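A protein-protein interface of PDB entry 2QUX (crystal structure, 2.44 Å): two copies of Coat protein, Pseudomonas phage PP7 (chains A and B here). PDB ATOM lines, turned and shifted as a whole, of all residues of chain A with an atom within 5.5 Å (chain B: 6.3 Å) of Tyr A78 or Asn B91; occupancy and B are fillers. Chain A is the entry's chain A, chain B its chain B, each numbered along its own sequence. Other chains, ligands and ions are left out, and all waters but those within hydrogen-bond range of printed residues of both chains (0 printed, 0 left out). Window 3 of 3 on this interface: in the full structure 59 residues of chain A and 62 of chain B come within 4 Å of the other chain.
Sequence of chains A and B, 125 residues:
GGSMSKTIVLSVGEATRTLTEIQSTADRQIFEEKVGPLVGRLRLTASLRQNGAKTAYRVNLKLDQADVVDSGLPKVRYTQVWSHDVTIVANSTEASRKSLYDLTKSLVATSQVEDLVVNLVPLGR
The backbone carbonyl oxygen of Ser B96 sits at hydrogen-bond distance from the side-chain amide nitrogen of Gln A65 (2.7 Å).
The backbone NH of Val B89 sits at hydrogen-bond distance from the side-chain amide oxygen of Gln A80 (2.9 Å).
The side-chain amide nitrogen (NE2) of Gln A80 is in hydrogen-bond range of the side-chain hydroxyl (OG) of Ser B96 (3.1 Å).
The side-chain hydroxyl of Ser B92 is in hydrogen-bond range of the side-chain amide oxygen of Gln A80, at 2.8 Å.
The backbone NH of Asp A67 is in hydrogen-bond range of the backbone carbonyl oxygen of Tyr A78 (2.8 Å).
The backbone carbonyl oxygen (O) of Val B89 is in hydrogen-bond range of the side-chain hydroxyl (OG) of Ser B92.
NH2 of Arg B97 lies within hydrogen-bond range of O of Val B89.
The side-chain hydroxyl (OG) of Ser B92 is in hydrogen-bond range of the guanidinium group (NE) of Arg B97 (3.1 Å).
The side-chain hydroxyl (OG) of Ser B96 lies within hydrogen-bond range of the backbone carbonyl oxygen (O) of Thr B93 (2.7 Å).
The backbone carbonyl oxygen (O) of Gln A80 sits at hydrogen-bond distance from the backbone NH (N) of Gln A65 (2.8 Å).
Among the printed residues, merely in contact across the chains: Tyr A78 with Ser B92, Thr A79 with Val B89, Tyr A78 with Thr B93, Tyr A78 with Val B89, Tyr A78 with Ser B96 and Tyr A78 with Asn B91.
Tyr A78 touches five residues of chain B.
Of chain A, only Tyr A78 (3.9 Å) comes within 4 Å of Asn B91.
Printed residues of chain A within 4 Å of Val B89: Tyr A78 (3.8 Å), Thr A79 (3.7 Å) and Gln A80 (2.9 Å).
Of the printed residues of chain B, Thr A79 touches Val B89 (3.7 Å).
Of the printed residues of chain A, Thr B93 touches Tyr A78.
The nearest printed residue of chain A that does not touch Asn B91 is Arg A77 (5.9 Å).
The nearest printed residue of chain A that does not touch Val B89 is Arg A77 (7.0 Å).
Printed residues of chain B that touch a printed residue of chain A: Val B89, Asn B91, Ser B92, Thr B93 and Ser B96.
No position is printed for both chains.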
ATOM      1  N   GLN A  65      11.744 -19.125 -30.257  1.00  0.00           N
ATOM      2  CA  GLN A  65      12.156 -17.736 -30.422  1.00  0.00           C
ATOM      3  C   GLN A  65      12.853 -17.184 -29.177  1.00  0.00           C
ATOM      4  O   GLN A  65      12.198 -16.804 -28.212  1.00  0.00           O
ATOM      5  CB  GLN A  65      10.966 -16.862 -30.770  1.00  0.00           C
ATOM      6  CG  GLN A  65      11.417 -15.462 -31.277  1.00  0.00           C
ATOM      7  CD  GLN A  65      10.264 -14.538 -31.483  1.00  0.00           C
ATOM      8  OE1 GLN A  65      10.000 -14.108 -32.599  1.00  0.00           O
ATOM      9  NE2 GLN A  65       9.547 -14.239 -30.406  1.00  0.00           N
ATOM     10  N   ALA A  66      14.183 -17.126 -29.231  1.00  0.00           N
ATOM     11  CA  ALA A  66      14.997 -16.654 -28.127  1.00  0.00           C
ATOM     12  C   ALA A  66      15.084 -15.138 -28.139  1.00  0.00           C
ATOM     13  O   ALA A  66      14.907 -14.494 -29.185  1.00  0.00           O
ATOM     14  CB  ALA A  66      16.387 -17.263 -28.195  1.00  0.00           C
ATOM     15  N   ASP A  67      15.341 -14.579 -26.958  1.00  0.00           N
ATOM     16  CA  ASP A  67      15.530 -13.158 -26.795  1.00  0.00           C
ATOM     17  C   ASP A  67      16.971 -12.919 -26.399  1.00  0.00           C
ATOM     18  O   ASP A  67      17.359 -13.260 -25.288  1.00  0.00           O
ATOM     19  CB  ASP A  67      14.582 -12.623 -25.737  1.00  0.00           C
ATOM     20  CG  ASP A  67      14.541 -11.123 -25.720  1.00  0.00           C
ATOM     21  OD1 ASP A  67      13.661 -10.572 -26.414  1.00  0.00           O
ATOM     22  OD2 ASP A  67      15.398 -10.508 -25.043  1.00  0.00           O
ATOM     23  N   VAL A  76      21.381 -15.243 -24.494  1.00  0.00           N
ATOM     24  CA  VAL A  76      19.939 -15.519 -24.519  1.00  0.00           C
ATOM     25  C   VAL A  76      19.324 -15.241 -23.135  1.00  0.00           C
ATOM     26  O   VAL A  76      19.699 -15.872 -22.153  1.00  0.00           O
ATOM     27  CB  VAL A  76      19.652 -16.987 -24.930  1.00  0.00           C
ATOM     28  CG1 VAL A  76      18.168 -17.297 -24.813  1.00  0.00           C
ATOM     29  CG2 VAL A  76      20.156 -17.264 -26.359  1.00  0.00           C
ATOM     30  N   ARG A  77      18.394 -14.291 -23.073  1.00  0.00           N
ATOM     31  CA  ARG A  77      17.717 -13.924 -21.829  1.00  0.00           C
ATOM     32  C   ARG A  77      16.602 -14.923 -21.489  1.00  0.00           C
ATOM     33  O   ARG A  77      16.540 -15.432 -20.374  1.00  0.00           O
ATOM     34  CB  ARG A  77      17.166 -12.499 -21.945  1.00  0.00           C
ATOM     35  CG  ARG A  77      16.720 -11.897 -20.618  1.00  0.00           C
ATOM     36  CD  ARG A  77      16.675 -10.380 -20.656  1.00  0.00           C
ATOM     37  NE  ARG A  77      15.757  -9.856 -21.674  1.00  0.00           N
ATOM     38  CZ  ARG A  77      15.426  -8.566 -21.825  1.00  0.00           C
ATOM     39  NH1 ARG A  77      14.584  -8.209 -22.800  1.00  0.00           N
ATOM     40  NH2 ARG A  77      15.917  -7.619 -21.016  1.00  0.00           N
ATOM     41  N   TYR A  78      15.728 -15.187 -22.459  1.00  0.00           N
ATOM     42  CA  TYR A  78      14.665 -16.201 -22.340  1.00  0.00           C
ATOM     43  C   TYR A  78      14.307 -16.755 -23.727  1.00  0.00           C
ATOM     44  O   TYR A  78      14.737 -16.199 -24.736  1.00  0.00           O
ATOM     45  CB  TYR A  78      13.421 -15.607 -21.646  1.00  0.00           C
ATOM     46  CG  TYR A  78      12.855 -14.328 -22.277  1.00  0.00           C
ATOM     47  CD1 TYR A  78      12.115 -14.366 -23.460  1.00  0.00           C
ATOM     48  CD2 TYR A  78      13.045 -13.086 -21.673  1.00  0.00           C
ATOM     49  CE1 TYR A  78      11.604 -13.210 -24.031  1.00  0.00           C
ATOM     50  CE2 TYR A  78      12.522 -11.916 -22.238  1.00  0.00           C
ATOM     51  CZ  TYR A  78      11.802 -11.983 -23.417  1.00  0.00           C
ATOM     52  OH  TYR A  78      11.275 -10.833 -23.999  1.00  0.00           O
ATOM     53  N   THR A  79      13.515 -17.831 -23.758  1.00  0.00           N
ATOM     54  CA  THR A  79      13.000 -18.429 -25.004  1.00  0.00           C
ATOM     55  C   THR A  79      11.487 -18.597 -24.878  1.00  0.00           C
ATOM     56  O   THR A  79      10.987 -18.968 -23.813  1.00  0.00           O
ATOM     57  CB  THR A  79      13.681 -19.795 -25.333  1.00  0.00           C
ATOM     58  OG1 THR A  79      15.094 -19.606 -25.480  1.00  0.00           O
ATOM     59  CG2 THR A  79      13.155 -20.392 -26.624  1.00  0.00           C
ATOM     60  N   GLN A  80      10.765 -18.256 -25.947  1.00  0.00           N
ATOM     61  CA  GLN A  80       9.313 -18.455 -26.026  1.00  0.00           C
ATOM     62  C   GLN A  80       9.109 -19.413 -27.168  1.00  0.00           C
ATOM     63  O   GLN A  80       9.900 -19.435 -28.118  1.00  0.00           O
ATOM     64  CB  GLN A  80       8.608 -17.141 -26.248  1.00  0.00           C
ATOM     65  CG  GLN A  80       8.867 -16.167 -25.120  1.00  0.00           C
ATOM     66  CD  GLN A  80       8.126 -14.857 -25.275  1.00  0.00           C
ATOM     67  OE1 GLN A  80       7.313 -14.482 -24.427  1.00  0.00           O
ATOM     68  NE2 GLN A  80       8.417 -14.145 -26.347  1.00  0.00           N
ATOM     69  N   THR B  55       6.864 -17.215 -13.642  1.00  0.00           N
ATOM     70  CA  THR B  55       7.662 -16.444 -14.598  1.00  0.00           C
ATOM     71  C   THR B  55       7.262 -16.683 -16.089  1.00  0.00           C
ATOM     72  O   THR B  55       7.903 -16.156 -16.993  1.00  0.00           O
ATOM     73  CB  THR B  55       9.139 -16.828 -14.433  1.00  0.00           C
ATOM     74  OG1 THR B  55       9.282 -18.236 -14.649  1.00  0.00           O
ATOM     75  CG2 THR B  55       9.641 -16.484 -13.026  1.00  0.00           C
ATOM     76  N   VAL B  89       6.792 -15.939 -21.961  1.00  0.00           N
ATOM     77  CA  VAL B  89       7.498 -15.426 -20.779  1.00  0.00           C
ATOM     78  C   VAL B  89       6.764 -14.185 -20.228  1.00  0.00           C
ATOM     79  O   VAL B  89       6.335 -13.326 -20.998  1.00  0.00           O
ATOM     80  CB  VAL B  89       8.958 -15.159 -21.100  1.00  0.00           C
ATOM     81  CG1 VAL B  89       9.661 -14.501 -19.923  1.00  0.00           C
ATOM     82  CG2 VAL B  89       9.630 -16.472 -21.474  1.00  0.00           C
ATOM     83  N   ALA B  90       6.591 -14.124 -18.907  1.00  0.00           N
ATOM     84  CA  ALA B  90       5.713 -13.133 -18.267  1.00  0.00           C
ATOM     85  C   ALA B  90       6.183 -11.709 -18.488  1.00  0.00           C
ATOM     86  O   ALA B  90       5.388 -10.844 -18.855  1.00  0.00           O
ATOM     87  CB  ALA B  90       5.578 -13.405 -16.759  1.00  0.00           C
ATOM     88  N   ASN B  91       7.478 -11.470 -18.291  1.00  0.00           N
ATOM     89  CA  ASN B  91       8.056 -10.124 -18.480  1.00  0.00           C
ATOM     90  C   ASN B  91       8.379  -9.729 -19.940  1.00  0.00           C
ATOM     91  O   ASN B  91       8.996  -8.688 -20.155  1.00  0.00           O
ATOM     92  CB  ASN B  91       9.294  -9.925 -17.568  1.00  0.00           C
ATOM     93  CG  ASN B  91      10.539 -10.718 -18.029  1.00  0.00           C
ATOM     94  OD1 ASN B  91      10.478 -11.578 -18.912  1.00  0.00           O
ATOM     95  ND2 ASN B  91      11.674 -10.426 -17.402  1.00  0.00           N
ATOM     96  N   SER B  92       7.961 -10.537 -20.925  1.00  0.00           N
ATOM     97  CA  SER B  92       8.357 -10.340 -22.304  1.00  0.00           C
ATOM     98  C   SER B  92       7.625  -9.173 -22.988  1.00  0.00           C
ATOM     99  O   SER B  92       6.573  -8.722 -22.531  1.00  0.00           O
ATOM    100  CB  SER B  92       8.193 -11.633 -23.099  1.00  0.00           C
ATOM    101  OG  SER B  92       6.849 -11.932 -23.385  1.00  0.00           O
ATOM    102  N   THR B  93       8.227  -8.669 -24.065  1.00  0.00           N
ATOM    103  CA  THR B  93       7.631  -7.609 -24.852  1.00  0.00           C
ATOM    104  C   THR B  93       6.460  -8.131 -25.671  1.00  0.00           C
ATOM    105  O   THR B  93       6.477  -9.270 -26.138  1.00  0.00           O
ATOM    106  CB  THR B  93       8.628  -6.947 -25.834  1.00  0.00           C
ATOM    107  OG1 THR B  93       9.102  -7.913 -26.784  1.00  0.00           O
ATOM    108  CG2 THR B  93       9.795  -6.301 -25.095  1.00  0.00           C
ATOM    109  N   SER B  96       7.757  -9.276 -29.046  1.00  0.00           N
ATOM    110  CA  SER B  96       8.285 -10.657 -29.076  1.00  0.00           C
ATOM    111  C   SER B  96       7.197 -11.705 -29.124  1.00  0.00           C
ATOM    112  O   SER B  96       7.352 -12.718 -29.793  1.00  0.00           O
ATOM    113  CB  SER B  96       9.202 -10.948 -27.869  1.00  0.00           C
ATOM    114  OG  SER B  96       8.475 -11.069 -26.658  1.00  0.00           O
ATOM    115  N   ARG B  97       6.098 -11.454 -28.414  1.00  0.00           N
ATOM    116  CA  ARG B  97       4.935 -12.345 -28.413  1.00  0.00           C
ATOM    117  C   ARG B  97       4.200 -12.294 -29.736  1.00  0.00           C
ATOM    118  O   ARG B  97       3.832 -13.329 -30.280  1.00  0.00           O
ATOM    119  CB  ARG B  97       3.959 -11.969 -27.308  1.00  0.00           C
ATOM    120  CG  ARG B  97       4.469 -12.052 -25.870  1.00  0.00           C
ATOM    121  CD  ARG B  97       3.395 -11.525 -24.921  1.00  0.00           C
ATOM    122  NE  ARG B  97       3.810 -11.552 -23.527  1.00  0.00           N
ATOM    123  CZ  ARG B  97       3.015 -11.368 -22.466  1.00  0.00           C
ATOM    124  NH1 ARG B  97       1.698 -11.193 -22.575  1.00  0.00           N
ATOM    125  NH2 ARG B  97       3.554 -11.411 -21.247  1.00  0.00           N
